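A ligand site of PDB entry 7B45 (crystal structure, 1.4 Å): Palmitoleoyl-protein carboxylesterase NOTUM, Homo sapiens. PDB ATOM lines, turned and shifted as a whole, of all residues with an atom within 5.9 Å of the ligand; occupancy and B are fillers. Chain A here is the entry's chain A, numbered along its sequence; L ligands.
A ring nitrogen (ND1) of His 312 sits at hydrogen-bond distance from the side-chain carboxylate (OD1) of Asp 263. NE2 of His 312 lies within hydrogen-bond range of OG of Ser 155 (2.7 Å). The side-chain carboxylate (OD2) of Asp 263 is in hydrogen-bond range of the backbone NH (N) of Ala 265 (2.9 Å). The backbone NH (N) of Val 110 sits at hydrogen-bond distance from the side-chain hydroxyl (OH) of Tyr 105 (2.9 Å). The side-chain hydroxyl of Tyr 105 is in hydrogen-bond range of the backbone carbonyl oxygen of Trp 51. OG1 of Thr 159 lies within hydrogen-bond range of O of Gly 189 (2.9 Å). N of Gly 49 sits close to O of Ser 154. The side-chain carboxylate (OE1) of Glu 313 sits at hydrogen-bond distance from the side-chain hydroxyl (OG) of Ser 155, 2.7 Å away.
Gly 49 touches the ligand. Tyr 52 touches the ligand (OH to C1, 3.2 Å). Val 110 touches the ligand. Ser 155 touches the ligand (CB to O1, 3.3 Å). Thr 159 touches the ligand. Phe 191 touches the ligand. CB of Pro 210 touches C1 of the ligand, 3.5 Å away. CD1 of Ile 214 touches C2 of the ligand, 3.1 Å away. O of Phe 242 touches C4 of the ligand, 3.2 Å away. Phe 243 touches the ligand (CZ to C3, 3.8 Å). Ala 265 touches the ligand (CB to N4, 3.3 Å). Hydrophobic or aromatic side chains that line the ligand: Trp 51, Tyr 52, Val 110, Ala 156, Phe 191, Pro 210, Ile 214, Phe 243, Ala 265 and His 312. The nearest printed residue that does not touch the ligand is Val 269 (4.6 Å).
An oxygen (O1) of the ligand lies within hydrogen-bond range of the backbone NH of Ala 156, at 3.1 Å. A ring nitrogen (NE2) of His 312 is in hydrogen-bond range of a nitrogen (N3) of the ligand (3.2 Å). N of Trp 51 is in hydrogen-bond range of O1 of the ligand, at 2.7 Å. O1 of the ligand sits at hydrogen-bond distance from N of Gly 50.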
ATOM      1  N   GLY A  49      20.563 -20.925 -10.120  1.00  0.00           N
ATOM      2  CA  GLY A  49      21.801 -20.205  -9.914  1.00  0.00           C
ATOM      3  C   GLY A  49      22.916 -20.670 -10.830  1.00  0.00           C
ATOM      4  O   GLY A  49      22.709 -21.398 -11.796  1.00  0.00           O
ATOM      5  N   GLY A  50      24.129 -20.221 -10.516  1.00  0.00           N
ATOM      6  CA  GLY A  50      25.289 -20.564 -11.312  1.00  0.00           C
ATOM      7  C   GLY A  50      26.264 -19.424 -11.575  1.00  0.00           C
ATOM      8  O   GLY A  50      26.727 -19.255 -12.715  1.00  0.00           O
ATOM      9  N   TRP A  51      26.599 -18.660 -10.551  1.00  0.00           N
ATOM     10  CA  TRP A  51      27.626 -17.597 -10.626  1.00  0.00           C
ATOM     11  C   TRP A  51      27.172 -16.545 -11.650  1.00  0.00           C
ATOM     12  O   TRP A  51      25.985 -16.192 -11.691  1.00  0.00           O
ATOM     13  CB  TRP A  51      29.036 -18.141 -10.782  1.00  0.00           C
ATOM     14  CG  TRP A  51      29.489 -18.864  -9.552  1.00  0.00           C
ATOM     15  CD1 TRP A  51      29.450 -20.206  -9.338  1.00  0.00           C
ATOM     16  CD2 TRP A  51      30.016 -18.272  -8.362  1.00  0.00           C
ATOM     17  NE1 TRP A  51      29.931 -20.497  -8.086  1.00  0.00           N
ATOM     18  CE2 TRP A  51      30.272 -19.323  -7.464  1.00  0.00           C
ATOM     19  CE3 TRP A  51      30.280 -16.961  -7.973  1.00  0.00           C
ATOM     20  CZ2 TRP A  51      30.809 -19.101  -6.193  1.00  0.00           C
ATOM     21  CZ3 TRP A  51      30.817 -16.739  -6.703  1.00  0.00           C
ATOM     22  CH2 TRP A  51      31.070 -17.810  -5.835  1.00  0.00           C
ATOM     23  N   TYR A  52      28.095 -15.997 -12.446  1.00  0.00           N
ATOM     24  CA  TYR A  52      27.840 -14.886 -13.358  1.00  0.00           C
ATOM     25  C   TYR A  52      29.121 -14.684 -14.135  1.00  0.00           C
ATOM     26  O   TYR A  52      30.153 -15.303 -13.844  1.00  0.00           O
ATOM     27  CB  TYR A  52      27.439 -13.591 -12.624  1.00  0.00           C
ATOM     28  CG  TYR A  52      28.426 -13.121 -11.595  1.00  0.00           C
ATOM     29  CD1 TYR A  52      29.419 -12.221 -11.930  1.00  0.00           C
ATOM     30  CD2 TYR A  52      28.372 -13.574 -10.285  1.00  0.00           C
ATOM     31  CE1 TYR A  52      30.341 -11.773 -10.990  1.00  0.00           C
ATOM     32  CE2 TYR A  52      29.276 -13.138  -9.336  1.00  0.00           C
ATOM     33  CZ  TYR A  52      30.256 -12.237  -9.698  1.00  0.00           C
ATOM     34  OH  TYR A  52      31.182 -11.790  -8.772  1.00  0.00           O
ATOM     35  N   TYR A 105      18.726 -20.377 -15.675  1.00  0.00           N
ATOM     36  CA  TYR A 105      19.588 -19.212 -15.581  1.00  0.00           C
ATOM     37  C   TYR A 105      20.475 -19.226 -16.806  1.00  0.00           C
ATOM     38  O   TYR A 105      21.420 -20.008 -16.904  1.00  0.00           O
ATOM     39  CB  TYR A 105      20.380 -19.330 -14.297  1.00  0.00           C
ATOM     40  CG  TYR A 105      21.346 -18.220 -13.996  1.00  0.00           C
ATOM     41  CD1 TYR A 105      20.984 -16.884 -14.166  1.00  0.00           C
ATOM     42  CD2 TYR A 105      22.584 -18.501 -13.424  1.00  0.00           C
ATOM     43  CE1 TYR A 105      21.869 -15.857 -13.835  1.00  0.00           C
ATOM     44  CE2 TYR A 105      23.447 -17.485 -13.070  1.00  0.00           C
ATOM     45  CZ  TYR A 105      23.094 -16.178 -13.289  1.00  0.00           C
ATOM     46  OH  TYR A 105      23.980 -15.182 -12.935  1.00  0.00           O
ATOM     47  N   VAL A 110      23.088 -12.476 -12.487  1.00  0.00           N
ATOM     48  CA  VAL A 110      22.454 -12.642 -11.173  1.00  0.00           C
ATOM     49  C   VAL A 110      21.002 -12.150 -11.330  1.00  0.00           C
ATOM     50  O   VAL A 110      20.401 -11.574 -10.404  1.00  0.00           O
ATOM     51  CB  VAL A 110      23.254 -11.859 -10.112  1.00  0.00           C
ATOM     52  CG1 VAL A 110      22.644 -11.934  -8.722  1.00  0.00           C
ATOM     53  CG2 VAL A 110      24.731 -12.180 -10.139  1.00  0.00           C
ATOM     54  N   SER A 154      17.924 -20.352  -5.819  1.00  0.00           N
ATOM     55  CA  SER A 154      19.110 -20.785  -5.094  1.00  0.00           C
ATOM     56  C   SER A 154      20.363 -20.113  -5.643  1.00  0.00           C
ATOM     57  O   SER A 154      20.519 -19.977  -6.864  1.00  0.00           O
ATOM     58  CB  SER A 154      19.296 -22.298  -5.134  1.00  0.00           C
ATOM     59  OG  SER A 154      18.217 -22.972  -4.460  1.00  0.00           O
ATOM     60  N   SER A 155      21.269 -19.717  -4.739  1.00  0.00           N
ATOM     61  CA  SER A 155      22.584 -19.143  -5.083  1.00  0.00           C
ATOM     62  C   SER A 155      22.375 -17.850  -5.843  1.00  0.00           C
ATOM     63  O   SER A 155      21.725 -16.936  -5.302  1.00  0.00           O
ATOM     64  CB  SER A 155      23.446 -20.199  -5.772  1.00  0.00           C
ATOM     65  OG  SER A 155      23.594 -21.334  -4.963  1.00  0.00           O
ATOM     66  N   ALA A 156      22.911 -17.688  -7.064  1.00  0.00           N
ATOM     67  CA  ALA A 156      22.616 -16.469  -7.824  1.00  0.00           C
ATOM     68  C   ALA A 156      21.114 -16.299  -7.994  1.00  0.00           C
ATOM     69  O   ALA A 156      20.626 -15.178  -8.075  1.00  0.00           O
ATOM     70  CB  ALA A 156      23.312 -16.511  -9.188  1.00  0.00           C
ATOM     71  N   GLY A 157      20.380 -17.410  -8.053  1.00  0.00           N
ATOM     72  CA  GLY A 157      18.931 -17.318  -8.103  1.00  0.00           C
ATOM     73  C   GLY A 157      18.314 -16.793  -6.811  1.00  0.00           C
ATOM     74  O   GLY A 157      17.267 -16.135  -6.838  1.00  0.00           O
ATOM     75  N   THR A 159      19.848 -14.580  -4.748  1.00  0.00           N
ATOM     76  CA  THR A 159      20.028 -13.141  -4.877  1.00  0.00           C
ATOM     77  C   THR A 159      19.029 -12.571  -5.888  1.00  0.00           C
ATOM     78  O   THR A 159      18.475 -11.482  -5.678  1.00  0.00           O
ATOM     79  CB  THR A 159      21.470 -12.823  -5.279  1.00  0.00           C
ATOM     80  OG1 THR A 159      22.370 -13.507  -4.384  1.00  0.00           O
ATOM     81  CG2 THR A 159      21.727 -11.331  -5.180  1.00  0.00           C
ATOM     82  N   SER A 188      20.434 -19.391  -0.160  1.00  0.00           N
ATOM     83  CA  SER A 188      21.869 -19.343  -0.419  1.00  0.00           C
ATOM     84  C   SER A 188      22.269 -18.146  -1.268  1.00  0.00           C
ATOM     85  O   SER A 188      23.225 -18.217  -2.046  1.00  0.00           O
ATOM     86  CB  SER A 188      22.366 -20.654  -1.032  1.00  0.00           C
ATOM     87  OG  SER A 188      22.112 -21.705  -0.102  1.00  0.00           O
ATOM     88  N   GLY A 189      21.527 -17.055  -1.143  1.00  0.00           N
ATOM     89  CA  GLY A 189      21.859 -15.850  -1.881  1.00  0.00           C
ATOM     90  C   GLY A 189      22.092 -14.640  -1.004  1.00  0.00           C
ATOM     91  O   GLY A 189      22.006 -13.503  -1.486  1.00  0.00           O
ATOM     92  N   PHE A 191      24.738 -12.913   1.051  1.00  0.00           N
ATOM     93  CA  PHE A 191      26.181 -12.854   1.212  1.00  0.00           C
ATOM     94  C   PHE A 191      26.619 -11.616   1.986  1.00  0.00           C
ATOM     95  O   PHE A 191      25.898 -10.614   2.080  1.00  0.00           O
ATOM     96  CB  PHE A 191      26.863 -12.887  -0.156  1.00  0.00           C
ATOM     97  CG  PHE A 191      26.555 -14.120  -0.917  1.00  0.00           C
ATOM     98  CD1 PHE A 191      27.047 -15.341  -0.501  1.00  0.00           C
ATOM     99  CD2 PHE A 191      25.673 -14.085  -1.986  1.00  0.00           C
ATOM    100  CE1 PHE A 191      26.723 -16.505  -1.177  1.00  0.00           C
ATOM    101  CE2 PHE A 191      25.348 -15.239  -2.662  1.00  0.00           C
ATOM    102  CZ  PHE A 191      25.862 -16.449  -2.268  1.00  0.00           C
ATOM    103  N   PRO A 210      35.253  -9.665  -5.067  1.00  0.00           N
ATOM    104  CA  PRO A 210      33.792  -9.844  -5.139  1.00  0.00           C
ATOM    105  C   PRO A 210      32.954  -8.607  -5.416  1.00  0.00           C
ATOM    106  O   PRO A 210      32.206  -8.576  -6.396  1.00  0.00           O
ATOM    107  CB  PRO A 210      33.489 -10.457  -3.757  1.00  0.00           C
ATOM    108  CG  PRO A 210      34.921 -10.779  -3.135  1.00  0.00           C
ATOM    109  CD  PRO A 210      35.817 -10.783  -4.320  1.00  0.00           C
ATOM    110  N   THR A 211      33.042  -7.572  -4.553  1.00  0.00           N
ATOM    111  CA  THR A 211      32.242  -6.374  -4.781  1.00  0.00           C
ATOM    112  C   THR A 211      32.661  -5.656  -6.055  1.00  0.00           C
ATOM    113  O   THR A 211      31.821  -5.029  -6.722  1.00  0.00           O
ATOM    114  CB  THR A 211      32.324  -5.420  -3.600  1.00  0.00           C
ATOM    115  OG1 THR A 211      33.683  -5.045  -3.380  1.00  0.00           O
ATOM    116  CG2 THR A 211      31.758  -6.053  -2.344  1.00  0.00           C
ATOM    117  N   ALA A 213      33.777  -7.111  -8.819  1.00  0.00           N
ATOM    118  CA  ALA A 213      33.249  -7.883  -9.937  1.00  0.00           C
ATOM    119  C   ALA A 213      31.782  -7.552 -10.184  1.00  0.00           C
ATOM    120  O   ALA A 213      31.339  -7.449 -11.329  1.00  0.00           O
ATOM    121  CB  ALA A 213      33.435  -9.377  -9.687  1.00  0.00           C
ATOM    122  N   ILE A 214      31.004  -7.373  -9.106  1.00  0.00           N
ATOM    123  CA  ILE A 214      29.606  -6.989  -9.277  1.00  0.00           C
ATOM    124  C   ILE A 214      29.481  -5.563  -9.791  1.00  0.00           C
ATOM    125  O   ILE A 214      28.624  -5.277 -10.632  1.00  0.00           O
ATOM    126  CB  ILE A 214      28.795  -7.202  -7.985  1.00  0.00           C
ATOM    127  CG1 ILE A 214      28.621  -8.681  -7.690  1.00  0.00           C
ATOM    128  CG2 ILE A 214      27.425  -6.547  -8.097  1.00  0.00           C
ATOM    129  CD1 ILE A 214      28.005  -8.846  -6.384  1.00  0.00           C
ATOM    130  N   PHE A 242      23.012  -5.915  -4.118  1.00  0.00           N
ATOM    131  CA  PHE A 242      23.208  -7.339  -4.311  1.00  0.00           C
ATOM    132  C   PHE A 242      23.497  -8.068  -3.010  1.00  0.00           C
ATOM    133  O   PHE A 242      23.574  -9.306  -3.001  1.00  0.00           O
ATOM    134  CB  PHE A 242      24.355  -7.582  -5.303  1.00  0.00           C
ATOM    135  CG  PHE A 242      23.977  -7.397  -6.739  1.00  0.00           C
ATOM    136  CD1 PHE A 242      23.543  -6.174  -7.217  1.00  0.00           C
ATOM    137  CD2 PHE A 242      24.092  -8.463  -7.625  1.00  0.00           C
ATOM    138  CE1 PHE A 242      23.215  -6.026  -8.577  1.00  0.00           C
ATOM    139  CE2 PHE A 242      23.764  -8.316  -8.962  1.00  0.00           C
ATOM    140  CZ  PHE A 242      23.326  -7.103  -9.427  1.00  0.00           C
ATOM    141  N   PHE A 243      23.632  -7.332  -1.918  1.00  0.00           N
ATOM    142  CA  PHE A 243      23.924  -7.921  -0.621  1.00  0.00           C
ATOM    143  C   PHE A 243      22.649  -7.943   0.206  1.00  0.00           C
ATOM    144  O   PHE A 243      22.078  -6.885   0.514  1.00  0.00           O
ATOM    145  CB  PHE A 243      25.061  -7.145   0.037  1.00  0.00           C
ATOM    146  CG  PHE A 243      26.362  -7.452  -0.629  1.00  0.00           C
ATOM    147  CD1 PHE A 243      27.113  -8.533  -0.222  1.00  0.00           C
ATOM    148  CD2 PHE A 243      26.750  -6.746  -1.765  1.00  0.00           C
ATOM    149  CE1 PHE A 243      28.273  -8.876  -0.884  1.00  0.00           C
ATOM    150  CE2 PHE A 243      27.910  -7.079  -2.426  1.00  0.00           C
ATOM    151  CZ  PHE A 243      28.669  -8.150  -1.979  1.00  0.00           C
ATOM    152  N   ASP A 263      28.380 -20.693   4.507  1.00  0.00           N
ATOM    153  CA  ASP A 263      28.086 -21.045   3.130  1.00  0.00           C
ATOM    154  C   ASP A 263      29.383 -21.232   2.352  1.00  0.00           C
ATOM    155  O   ASP A 263      30.304 -20.425   2.446  1.00  0.00           O
ATOM    156  CB  ASP A 263      27.240 -19.928   2.512  1.00  0.00           C
ATOM    157  CG  ASP A 263      26.876 -20.212   1.090  1.00  0.00           C
ATOM    158  OD1 ASP A 263      25.813 -20.816   0.861  1.00  0.00           O
ATOM    159  OD2 ASP A 263      27.658 -19.820   0.200  1.00  0.00           O
ATOM    160  N   ALA A 265      30.071 -20.954  -0.814  1.00  0.00           N
ATOM    161  CA  ALA A 265      30.392 -19.900  -1.766  1.00  0.00           C
ATOM    162  C   ALA A 265      30.896 -18.649  -1.059  1.00  0.00           C
ATOM    163  O   ALA A 265      31.795 -17.962  -1.577  1.00  0.00           O
ATOM    164  CB  ALA A 265      29.157 -19.579  -2.621  1.00  0.00           C
ATOM    165  N   GLN A 266      30.332 -18.321   0.099  1.00  0.00           N
ATOM    166  CA  GLN A 266      30.869 -17.219   0.904  1.00  0.00           C
ATOM    167  C   GLN A 266      32.317 -17.501   1.272  1.00  0.00           C
ATOM    168  O   GLN A 266      33.195 -16.635   1.129  1.00  0.00           O
ATOM    169  CB  GLN A 266      30.021 -17.063   2.174  1.00  0.00           C
ATOM    170  CG  GLN A 266      30.513 -15.963   3.114  1.00  0.00           C
ATOM    171  CD  GLN A 266      30.144 -14.576   2.622  1.00  0.00           C
ATOM    172  OE1 GLN A 266      28.965 -14.304   2.344  1.00  0.00           O
ATOM    173  NE2 GLN A 266      31.123 -13.666   2.574  1.00  0.00           N
ATOM    174  N   VAL A 269      34.639 -17.016  -1.831  1.00  0.00           N
ATOM    175  CA  VAL A 269      34.987 -15.641  -2.166  1.00  0.00           C
ATOM    176  C   VAL A 269      35.870 -15.025  -1.088  1.00  0.00           C
ATOM    177  O   VAL A 269      36.676 -14.132  -1.373  1.00  0.00           O
ATOM    178  CB  VAL A 269      33.753 -14.790  -2.506  1.00  0.00           C
ATOM    179  CG1 VAL A 269      33.004 -15.390  -3.696  1.00  0.00           C
ATOM    180  CG2 VAL A 269      32.842 -14.617  -1.294  1.00  0.00           C
ATOM    181  N   HIS A 312      25.997 -25.592   0.731  1.00  0.00           N
ATOM    182  CA  HIS A 312      25.600 -24.617  -0.276  1.00  0.00           C
ATOM    183  C   HIS A 312      24.340 -25.098  -0.978  1.00  0.00           C
ATOM    184  O   HIS A 312      24.309 -26.220  -1.489  1.00  0.00           O
ATOM    185  CB  HIS A 312      26.719 -24.392  -1.308  1.00  0.00           C
ATOM    186  CG  HIS A 312      26.445 -23.241  -2.234  1.00  0.00           C
ATOM    187  ND1 HIS A 312      26.165 -21.972  -1.773  1.00  0.00           N
ATOM    188  CD2 HIS A 312      26.376 -23.194  -3.575  1.00  0.00           C
ATOM    189  CE1 HIS A 312      25.950 -21.180  -2.810  1.00  0.00           C
ATOM    190  NE2 HIS A 312      26.073 -21.895  -3.920  1.00  0.00           N
ATOM    191  N   GLU A 313      23.320 -24.229  -1.023  1.00  0.00           N
ATOM    192  CA  GLU A 313      21.979 -24.503  -1.556  1.00  0.00           C
ATOM    193  C   GLU A 313      21.246 -25.513  -0.689  1.00  0.00           C
ATOM    194  O   GLU A 313      21.889 -26.268   0.044  1.00  0.00           O
ATOM    195  CB  GLU A 313      22.025 -24.961  -3.023  1.00  0.00           C
ATOM    196  CG  GLU A 313      22.601 -23.917  -3.957  1.00  0.00           C
ATOM    197  CD  GLU A 313      22.624 -24.346  -5.424  1.00  0.00           C
ATOM    198  OE1 GLU A 313      22.655 -23.454  -6.296  1.00  0.00           O
ATOM    199  OE2 GLU A 313      22.606 -25.567  -5.693  1.00  0.00           O
HETATM  200  C1  LIG L   1      30.821 -11.865  -5.583  1.00  0.00           C
HETATM  201  C2  LIG L   1      28.087 -11.445  -4.663  1.00  0.00           C
HETATM  202  C3  LIG L   1      27.046 -10.937  -3.908  1.00  0.00           C
HETATM  203  C4  LIG L   1      25.750 -11.329  -4.203  1.00  0.00           C
HETATM  204  C5  LIG L   1      25.487 -12.220  -5.228  1.00  0.00           C
HETATM  205  C6  LIG L   1      26.532 -12.709  -5.997  1.00  0.00           C
HETATM  206  C7  LIG L   1      27.836 -12.316  -5.705  1.00  0.00           C
HETATM  207  C8  LIG L   1      26.759 -15.452  -6.659  1.00  0.00           C
HETATM  208  C9  LIG L   1      26.187 -19.027  -7.242  1.00  0.00           C
HETATM  209  C10 LIG L   1      27.427 -17.927  -5.680  1.00  0.00           C
HETATM  210  C11 LIG L   1      27.955 -16.815  -5.049  1.00  0.00           C
HETATM  211  C12 LIG L   1      27.627 -15.557  -5.536  1.00  0.00           C
HETATM  212  N1  LIG L   1      26.261 -16.512  -7.250  1.00  0.00           N
HETATM  213  N2  LIG L   1      26.610 -17.739  -6.740  1.00  0.00           N
HETATM  214  N3  LIG L   1      26.778 -20.035  -6.432  1.00  0.00           N
HETATM  215  N4  LIG L   1      27.540 -19.394  -5.461  1.00  0.00           N
HETATM  216  O1  LIG L   1      25.450 -19.147  -8.145  1.00  0.00           O
HETATM  217  S1  LIG L   1      29.826 -10.955  -4.367  1.00  0.00           S
HETATM  218  S2  LIG L   1      26.248 -13.881  -7.352  1.00  0.00           S
